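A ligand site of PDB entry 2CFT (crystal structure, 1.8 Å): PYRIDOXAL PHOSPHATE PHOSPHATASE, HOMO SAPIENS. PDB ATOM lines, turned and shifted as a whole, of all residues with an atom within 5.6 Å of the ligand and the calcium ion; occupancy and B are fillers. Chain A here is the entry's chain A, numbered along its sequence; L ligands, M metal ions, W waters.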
ATOM      1  N   ASP A  27     -21.891  10.701  -6.032  1.00  0.00           N
ATOM      2  CA  ASP A  27     -22.143   9.707  -4.989  1.00  0.00           C
ATOM      3  C   ASP A  27     -20.811   8.891  -4.912  1.00  0.00           C
ATOM      4  O   ASP A  27     -19.972   8.972  -5.831  1.00  0.00           O
ATOM      5  CB  ASP A  27     -23.355   8.913  -5.455  1.00  0.00           C
ATOM      6  CG  ASP A  27     -23.529   7.595  -4.762  1.00  0.00           C
ATOM      7  OD1 ASP A  27     -23.297   7.485  -3.530  1.00  0.00           O
ATOM      8  OD2 ASP A  27     -24.017   6.675  -5.469  1.00  0.00           O
ATOM      9  N   CYS A  28     -20.597   8.180  -3.808  1.00  0.00           N
ATOM     10  CA  CYS A  28     -19.314   7.574  -3.527  1.00  0.00           C
ATOM     11  C   CYS A  28     -19.339   6.057  -3.678  1.00  0.00           C
ATOM     12  O   CYS A  28     -18.788   5.512  -4.642  1.00  0.00           O
ATOM     13  CB  CYS A  28     -18.843   8.034  -2.135  1.00  0.00           C
ATOM     14  SG  CYS A  28     -18.653   9.855  -2.118  1.00  0.00           S
ATOM     15  N   ASP A  29     -20.022   5.347  -2.780  1.00  0.00           N
ATOM     16  CA  ASP A  29     -19.983   3.900  -2.873  1.00  0.00           C
ATOM     17  C   ASP A  29     -20.780   3.483  -4.119  1.00  0.00           C
ATOM     18  O   ASP A  29     -21.844   4.064  -4.405  1.00  0.00           O
ATOM     19  CB  ASP A  29     -20.598   3.257  -1.634  1.00  0.00           C
ATOM     20  CG  ASP A  29     -20.607   1.747  -1.737  1.00  0.00           C
ATOM     21  OD1 ASP A  29     -19.471   1.168  -1.783  1.00  0.00           O
ATOM     22  OD2 ASP A  29     -21.720   1.178  -1.889  1.00  0.00           O
ATOM     23  N   GLY A  30     -20.255   2.501  -4.849  1.00  0.00           N
ATOM     24  CA  GLY A  30     -20.881   2.048  -6.100  1.00  0.00           C
ATOM     25  C   GLY A  30     -20.497   2.888  -7.313  1.00  0.00           C
ATOM     26  O   GLY A  30     -20.836   2.542  -8.446  1.00  0.00           O
ATOM     27  N   VAL A  31     -19.737   3.960  -7.086  1.00  0.00           N
ATOM     28  CA  VAL A  31     -19.459   4.963  -8.121  1.00  0.00           C
ATOM     29  C   VAL A  31     -17.956   5.141  -8.226  1.00  0.00           C
ATOM     30  O   VAL A  31     -17.370   4.850  -9.260  1.00  0.00           O
ATOM     31  CB  VAL A  31     -20.106   6.332  -7.787  1.00  0.00           C
ATOM     32  CG1 VAL A  31     -19.733   7.411  -8.871  1.00  0.00           C
ATOM     33  CG2 VAL A  31     -21.630   6.192  -7.656  1.00  0.00           C
ATOM     34  N   VAL A  59     -20.886  13.426  -2.415  1.00  0.00           N
ATOM     35  CA  VAL A  59     -22.023  13.346  -1.507  1.00  0.00           C
ATOM     36  C   VAL A  59     -22.314  11.885  -1.158  1.00  0.00           C
ATOM     37  O   VAL A  59     -22.703  11.092  -2.021  1.00  0.00           O
ATOM     38  CB  VAL A  59     -23.291  14.065  -2.103  1.00  0.00           C
ATOM     39  CG1 VAL A  59     -23.617  13.609  -3.518  1.00  0.00           C
ATOM     40  CG2 VAL A  59     -24.501  13.976  -1.150  1.00  0.00           C
ATOM     41  N   SER A  60     -22.084  11.540   0.111  1.00  0.00           N
ATOM     42  CA  SER A  60     -22.293  10.160   0.577  1.00  0.00           C
ATOM     43  C   SER A  60     -23.285  10.102   1.733  1.00  0.00           C
ATOM     44  O   SER A  60     -23.196  10.907   2.652  1.00  0.00           O
ATOM     45  CB  SER A  60     -20.981   9.583   1.068  1.00  0.00           C
ATOM     46  OG  SER A  60     -21.119   8.203   1.436  1.00  0.00           O
ATOM     47  N   ASN A  61     -24.167   9.097   1.711  1.00  0.00           N
ATOM     48  CA  ASN A  61     -25.072   8.849   2.838  1.00  0.00           C
ATOM     49  C   ASN A  61     -24.388   8.134   4.002  1.00  0.00           C
ATOM     50  O   ASN A  61     -25.021   7.862   5.043  1.00  0.00           O
ATOM     51  CB  ASN A  61     -26.304   8.050   2.359  1.00  0.00           C
ATOM     52  CG  ASN A  61     -27.432   8.989   1.853  1.00  0.00           C
ATOM     53  OD1 ASN A  61     -27.272  10.210   1.887  1.00  0.00           O
ATOM     54  ND2 ASN A  61     -28.510   8.413   1.328  1.00  0.00           N
ATOM     55  N   ASN A  62     -23.110   7.833   3.843  1.00  0.00           N
ATOM     56  CA  ASN A  62     -22.390   7.058   4.845  1.00  0.00           C
ATOM     57  C   ASN A  62     -22.276   7.898   6.111  1.00  0.00           C
ATOM     58  O   ASN A  62     -21.703   8.988   6.065  1.00  0.00           O
ATOM     59  CB  ASN A  62     -21.006   6.642   4.334  1.00  0.00           C
ATOM     60  CG  ASN A  62     -20.434   5.452   5.093  1.00  0.00           C
ATOM     61  OD1 ASN A  62     -20.609   5.347   6.297  1.00  0.00           O
ATOM     62  ND2 ASN A  62     -19.767   4.529   4.385  1.00  0.00           N
ATOM     63  N   SER A  63     -22.856   7.409   7.206  1.00  0.00           N
ATOM     64  CA  SER A  63     -22.787   8.094   8.503  1.00  0.00           C
ATOM     65  C   SER A  63     -21.690   7.522   9.403  1.00  0.00           C
ATOM     66  O   SER A  63     -21.642   7.843  10.569  1.00  0.00           O
ATOM     67  CB  SER A  63     -24.137   7.991   9.237  1.00  0.00           C
ATOM     68  OG  SER A  63     -24.557   6.627   9.371  1.00  0.00           O
ATOM     69  N   ARG A  64     -20.811   6.685   8.863  1.00  0.00           N
ATOM     70  CA  ARG A  64     -19.775   6.046   9.713  1.00  0.00           C
ATOM     71  C   ARG A  64     -18.609   6.950  10.054  1.00  0.00           C
ATOM     72  O   ARG A  64     -18.045   6.826  11.137  1.00  0.00           O
ATOM     73  CB  ARG A  64     -19.217   4.767   9.093  1.00  0.00           C
ATOM     74  CG  ARG A  64     -20.009   3.525   9.459  1.00  0.00           C
ATOM     75  CD  ARG A  64     -19.346   2.303   8.865  1.00  0.00           C
ATOM     76  NE  ARG A  64     -19.368   1.155   9.759  1.00  0.00           N
ATOM     77  CZ  ARG A  64     -18.527   0.950  10.769  1.00  0.00           C
ATOM     78  NH1 ARG A  64     -17.567   1.838  11.035  1.00  0.00           N
ATOM     79  NH2 ARG A  64     -18.638  -0.122  11.524  1.00  0.00           N
ATOM     80  N   ARG A  73      -9.946   8.351   3.642  1.00  0.00           N
ATOM     81  CA  ARG A  73     -10.458   7.287   2.765  1.00  0.00           C
ATOM     82  C   ARG A  73     -10.392   7.628   1.264  1.00  0.00           C
ATOM     83  O   ARG A  73      -9.991   6.803   0.440  1.00  0.00           O
ATOM     84  CB  ARG A  73     -11.875   6.870   3.190  1.00  0.00           C
ATOM     85  CG  ARG A  73     -12.521   5.822   2.253  1.00  0.00           C
ATOM     86  CD  ARG A  73     -13.810   5.306   2.871  1.00  0.00           C
ATOM     87  NE  ARG A  73     -14.624   4.452   1.971  1.00  0.00           N
ATOM     88  CZ  ARG A  73     -14.310   3.191   1.673  1.00  0.00           C
ATOM     89  NH1 ARG A  73     -13.214   2.641   2.155  1.00  0.00           N
ATOM     90  NH2 ARG A  73     -15.103   2.470   0.867  1.00  0.00           N
ATOM     91  N   TYR A 152     -26.308   4.982  11.259  1.00  0.00           N
ATOM     92  CA  TYR A 152     -25.898   3.583  11.150  1.00  0.00           C
ATOM     93  C   TYR A 152     -25.337   3.161  12.509  1.00  0.00           C
ATOM     94  O   TYR A 152     -24.306   3.680  12.974  1.00  0.00           O
ATOM     95  CB  TYR A 152     -24.858   3.445  10.040  1.00  0.00           C
ATOM     96  CG  TYR A 152     -24.368   2.024   9.886  1.00  0.00           C
ATOM     97  CD1 TYR A 152     -25.073   1.096   9.116  1.00  0.00           C
ATOM     98  CD2 TYR A 152     -23.171   1.629  10.479  1.00  0.00           C
ATOM     99  CE1 TYR A 152     -24.606  -0.203   8.963  1.00  0.00           C
ATOM    100  CE2 TYR A 152     -22.704   0.305  10.324  1.00  0.00           C
ATOM    101  CZ  TYR A 152     -23.425  -0.583   9.567  1.00  0.00           C
ATOM    102  OH  TYR A 152     -22.963  -1.865   9.383  1.00  0.00           O
ATOM    103  N   ASP A 179     -30.163   8.875   6.913  1.00  0.00           N
ATOM    104  CA  ASP A 179     -30.493   8.403   5.577  1.00  0.00           C
ATOM    105  C   ASP A 179     -31.464   7.241   5.697  1.00  0.00           C
ATOM    106  O   ASP A 179     -31.680   6.737   6.807  1.00  0.00           O
ATOM    107  CB  ASP A 179     -29.207   7.930   4.850  1.00  0.00           C
ATOM    108  CG  ASP A 179     -28.575   6.691   5.491  1.00  0.00           C
ATOM    109  OD1 ASP A 179     -28.847   5.540   5.002  1.00  0.00           O
ATOM    110  OD2 ASP A 179     -27.874   6.814   6.524  1.00  0.00           O
ATOM    111  N   ASP A 181     -31.114   4.498   3.432  1.00  0.00           N
ATOM    112  CA  ASP A 181     -30.612   3.384   2.607  1.00  0.00           C
ATOM    113  C   ASP A 181     -30.940   2.069   3.336  1.00  0.00           C
ATOM    114  O   ASP A 181     -30.609   1.925   4.521  1.00  0.00           O
ATOM    115  CB  ASP A 181     -29.088   3.446   2.383  1.00  0.00           C
ATOM    116  CG  ASP A 181     -28.638   4.701   1.574  1.00  0.00           C
ATOM    117  OD1 ASP A 181     -27.422   4.849   1.363  1.00  0.00           O
ATOM    118  OD2 ASP A 181     -29.492   5.498   1.176  1.00  0.00           O
ATOM    119  N   HIS A 184     -26.584  -2.354   2.514  1.00  0.00           N
ATOM    120  CA  HIS A 184     -25.415  -2.082   1.634  1.00  0.00           C
ATOM    121  C   HIS A 184     -24.683  -3.358   1.329  1.00  0.00           C
ATOM    122  O   HIS A 184     -24.447  -4.158   2.243  1.00  0.00           O
ATOM    123  CB  HIS A 184     -24.456  -1.117   2.310  1.00  0.00           C
ATOM    124  CG  HIS A 184     -25.139   0.133   2.782  1.00  0.00           C
ATOM    125  ND1 HIS A 184     -25.436   1.158   1.907  1.00  0.00           N
ATOM    126  CD2 HIS A 184     -25.648   0.483   3.981  1.00  0.00           C
ATOM    127  CE1 HIS A 184     -26.085   2.112   2.571  1.00  0.00           C
ATOM    128  NE2 HIS A 184     -26.206   1.729   3.833  1.00  0.00           N
ATOM    129  N   THR A 192     -25.021  -5.600   4.693  1.00  0.00           N
ATOM    130  CA  THR A 192     -25.185  -5.105   6.051  1.00  0.00           C
ATOM    131  C   THR A 192     -26.499  -4.312   6.059  1.00  0.00           C
ATOM    132  O   THR A 192     -26.808  -3.615   5.082  1.00  0.00           O
ATOM    133  CB  THR A 192     -23.999  -4.248   6.558  1.00  0.00           C
ATOM    134  OG1 THR A 192     -24.135  -4.028   7.960  1.00  0.00           O
ATOM    135  CG2 THR A 192     -23.939  -2.887   5.878  1.00  0.00           C
ATOM    136  N   THR A 195     -29.170   2.234   7.536  1.00  0.00           N
ATOM    137  CA  THR A 195     -29.865   3.108   8.477  1.00  0.00           C
ATOM    138  C   THR A 195     -31.386   3.054   8.252  1.00  0.00           C
ATOM    139  O   THR A 195     -32.153   3.196   9.204  1.00  0.00           O
ATOM    140  CB  THR A 195     -29.341   4.567   8.363  1.00  0.00           C
ATOM    141  OG1 THR A 195     -27.932   4.576   8.583  1.00  0.00           O
ATOM    142  CG2 THR A 195     -30.013   5.472   9.386  1.00  0.00           C
ATOM    143  N   LYS A 215     -29.360  12.045   1.003  1.00  0.00           N
ATOM    144  CA  LYS A 215     -30.049  11.745  -0.258  1.00  0.00           C
ATOM    145  C   LYS A 215     -31.173  10.716   0.003  1.00  0.00           C
ATOM    146  O   LYS A 215     -30.964   9.745   0.759  1.00  0.00           O
ATOM    147  CB  LYS A 215     -29.043  11.109  -1.243  1.00  0.00           C
ATOM    148  CG  LYS A 215     -27.744  11.921  -1.392  1.00  0.00           C
ATOM    149  CD  LYS A 215     -26.732  11.129  -2.274  1.00  0.00           C
ATOM    150  CE  LYS A 215     -26.133   9.949  -1.507  1.00  0.00           C
ATOM    151  NZ  LYS A 215     -25.082   9.210  -2.323  1.00  0.00           N
ATOM    152  N   ASP A 240     -25.273   5.406  -8.096  1.00  0.00           N
ATOM    153  CA  ASP A 240     -25.586   4.013  -8.412  1.00  0.00           C
ATOM    154  C   ASP A 240     -26.949   3.541  -7.879  1.00  0.00           C
ATOM    155  O   ASP A 240     -27.312   2.378  -8.093  1.00  0.00           O
ATOM    156  CB  ASP A 240     -24.500   3.078  -7.844  1.00  0.00           C
ATOM    157  CG  ASP A 240     -24.606   2.938  -6.314  1.00  0.00           C
ATOM    158  OD1 ASP A 240     -24.869   3.965  -5.660  1.00  0.00           O
ATOM    159  OD2 ASP A 240     -24.401   1.829  -5.773  1.00  0.00           O
ATOM    160  N   ARG A 241     -27.692   4.394  -7.166  1.00  0.00           N
ATOM    161  CA  ARG A 241     -28.953   3.958  -6.573  1.00  0.00           C
ATOM    162  C   ARG A 241     -30.132   4.805  -7.098  1.00  0.00           C
ATOM    163  O   ARG A 241     -30.156   6.014  -6.904  1.00  0.00           O
ATOM    164  CB  ARG A 241     -28.845   4.045  -5.019  1.00  0.00           C
ATOM    165  CG  ARG A 241     -28.200   2.825  -4.322  1.00  0.00           C
ATOM    166  CD  ARG A 241     -28.540   2.723  -2.797  1.00  0.00           C
ATOM    167  NE  ARG A 241     -29.401   1.586  -2.393  1.00  0.00           N
ATOM    168  CZ  ARG A 241     -29.094   0.710  -1.427  1.00  0.00           C
ATOM    169  NH1 ARG A 241     -27.968   0.868  -0.742  1.00  0.00           N
ATOM    170  NH2 ARG A 241     -29.905  -0.314  -1.106  1.00  0.00           N
ATOM    171  N   ASP A 245     -29.846   8.336  -5.328  1.00  0.00           N
ATOM    172  CA  ASP A 245     -29.107   9.350  -6.083  1.00  0.00           C
ATOM    173  C   ASP A 245     -29.857   9.911  -7.268  1.00  0.00           C
ATOM    174  O   ASP A 245     -29.724  11.109  -7.574  1.00  0.00           O
ATOM    175  CB  ASP A 245     -27.808   8.733  -6.586  1.00  0.00           C
ATOM    176  CG  ASP A 245     -27.097   8.003  -5.495  1.00  0.00           C
ATOM    177  OD1 ASP A 245     -26.574   8.699  -4.606  1.00  0.00           O
ATOM    178  OD2 ASP A 245     -27.134   6.756  -5.473  1.00  0.00           O
HETATM  179  N1  LIG L   1     -24.061   4.068   4.779  1.00  0.00           N
HETATM  180  C1  LIG L   1     -23.327   3.004   5.253  1.00  0.00           C
HETATM  181  C2  LIG L   1     -23.478   2.576   6.688  1.00  0.00           C
HETATM  182  C3  LIG L   1     -22.445   2.311   4.413  1.00  0.00           C
HETATM  183  O1  LIG L   1     -21.567   1.388   4.929  1.00  0.00           O
HETATM  184  C4  LIG L   1     -22.312   2.693   3.088  1.00  0.00           C
HETATM  185  C5  LIG L   1     -21.327   2.003   2.182  1.00  0.00           C
HETATM  186  O2  LIG L   1     -20.293   1.547   2.680  1.00  0.00           O
HETATM  187  C6  LIG L   1     -23.045   3.753   2.592  1.00  0.00           C
HETATM  188  C7  LIG L   1     -23.913   4.459   3.444  1.00  0.00           C
HETATM  189  C8  LIG L   1     -22.543   4.281   1.241  1.00  0.00           C
HETATM  190  O3  LIG L   1     -23.208   5.475   0.949  1.00  0.00           O
HETATM  191  P1  LIG L   1     -23.054   6.157  -0.486  1.00  0.00           P
HETATM  192  O4  LIG L   1     -23.415   5.119  -1.518  1.00  0.00           O
HETATM  193  O5  LIG L   1     -21.641   6.698  -0.662  1.00  0.00           O
HETATM  194  O6  LIG L   1     -24.120   7.231  -0.436  1.00  0.00           O
HETATM  195 CA    CA M   1     -23.949   4.914  -3.701  1.00  0.00          CA
HETATM  196  O   HOH W   1     -17.955   2.001   4.981  1.00  0.00           O
HETATM  197  O   HOH W   2     -26.686   6.477  -0.757  1.00  0.00           O
HETATM  198  O   HOH W   3     -24.420   2.612  -3.119  1.00  0.00           O
HETATM  199  O   HOH W   4     -25.434   5.637   6.957  1.00  0.00           O
HETATM  200  O   HOH W   5     -18.149   1.054   1.027  1.00  0.00           O
HETATM  201  O   HOH W   6     -25.698   3.294  -0.551  1.00  0.00           O
HETATM  202  O   HOH W   7     -26.169   5.590  -3.163  1.00  0.00           O
HETATM  203  O   HOH W   8     -21.145  -0.832   0.843  1.00  0.00           O
HETATM  204  O   HOH W   9     -27.287   3.458   5.787  1.00  0.00           O
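Three residues have an atom within 4 Å of the calcium ion: Asp 27, Asp 29 and Asp 240. The nearest printed residue that does not touch the calcium ion is Asp 245 (4.1 Å).
Water W3 bridges the side-chain carboxylate of Asp 240 and the side-chain carboxylate of Asp 29. Water W5 lies within hydrogen-bond range of an oxygen (O2) of the ligand (2.8 Å), the side-chain carboxylate of Asp 29 (3.1 Å) and the guanidinium group of Arg 73 (3.4 Å). Water W6 lies within hydrogen-bond range of OD1 of Asp 181 (3.0 Å), ND1 of His 184 (3.3 Å) and NH1 of Arg 241 (3.3 Å). Water W8 lies within hydrogen-bond range of an oxygen (O2) of the ligand (3.1 Å) and the side-chain carboxylate of Asp 29 (3.4 Å). Water W1 bridges the side-chain amide nitrogen of Asn 62 (3.2 Å) and an oxygen (O2) of the ligand (3.3 Å). Water W9 lies within hydrogen-bond range of OD1 of Asp 179 (2.7 Å), NE2 of His 184 (2.8 Å), N of Thr 195 (2.8 Å) and N1 of the ligand (3.4 Å).
The backbone NH (N) of Asp 240 lies within hydrogen-bond range of the side-chain carboxylate (OD2) of Asp 245 (3.5 Å). The side-chain amide nitrogen of Asn 61 lies within hydrogen-bond range of the backbone carbonyl oxygen of Lys 215 (2.8 Å). The side-chain hydroxyl (OH) of Tyr 152 sits at hydrogen-bond distance from the side-chain hydroxyl (OG1) of Thr 192. The backbone NH of Tyr 152 is in hydrogen-bond range of the side-chain hydroxyl of Ser 63 (3.1 Å). NZ of Lys 215 is in hydrogen-bond range of O of Val 59, at 3.0 Å. The backbone NH (N) of Tyr 152 is in hydrogen-bond range of the side-chain hydroxyl (OG1) of Thr 195, at 3.2 Å. The side-chain amide oxygen of Asn 62 sits at hydrogen-bond distance from the backbone NH of Arg 64, 2.9 Å away. The side-chain amino group (NZ) of Lys 215 lies close to the side-chain carboxylate (OD1) of Asp 27, 2.8 Å away.
N of Asn 61 lies within hydrogen-bond range of O6 of the ligand (2.8 Å). N of Asp 29 sits at hydrogen-bond distance from O5 of the ligand (3.0 Å). NE2 of His 184 sits at hydrogen-bond distance from N1 of the ligand. The side-chain hydroxyl (OG) of Ser 60 is in hydrogen-bond range of an oxygen (O5) of the ligand. The side-chain amino group of Lys 215 is in salt-bridge range of an oxygen (O6) of the ligand. The side-chain amide nitrogen (ND2) of Asn 62 lies close to an oxygen (O2) of the ligand, 3.5 Å away.
The calcium ion is bound by an oxygen (O4) of the ligand (2.3 Å), the side-chain carboxylate (OD1) of Asp 240 (2.4 Å), the backbone carbonyl oxygen (O) of Asp 29 (2.4 Å), water W7 (2.4 Å), water W3 (2.4 Å), the side-chain carboxylate (OD2) of Asp 27 (2.5 Å) and the side-chain carboxylate (OD1) of Asp 27 (2.7 Å). The calcium ion has seven donor atoms within binding distance.
Residues that only touch the ligand: Cys 28 and Tyr 152. Hydrophobic or aromatic side chains within 4 Å of the ligand: Tyr 152 and His 184. Within 4 Å of the ligand: Asp 27, Cys 28, Asp 29, Ser 60, Asn 61, Asn 62, Tyr 152, His 184 and Lys 215. The nearest printed residue that does not touch the ligand is Asp 181 (4.1 Å).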
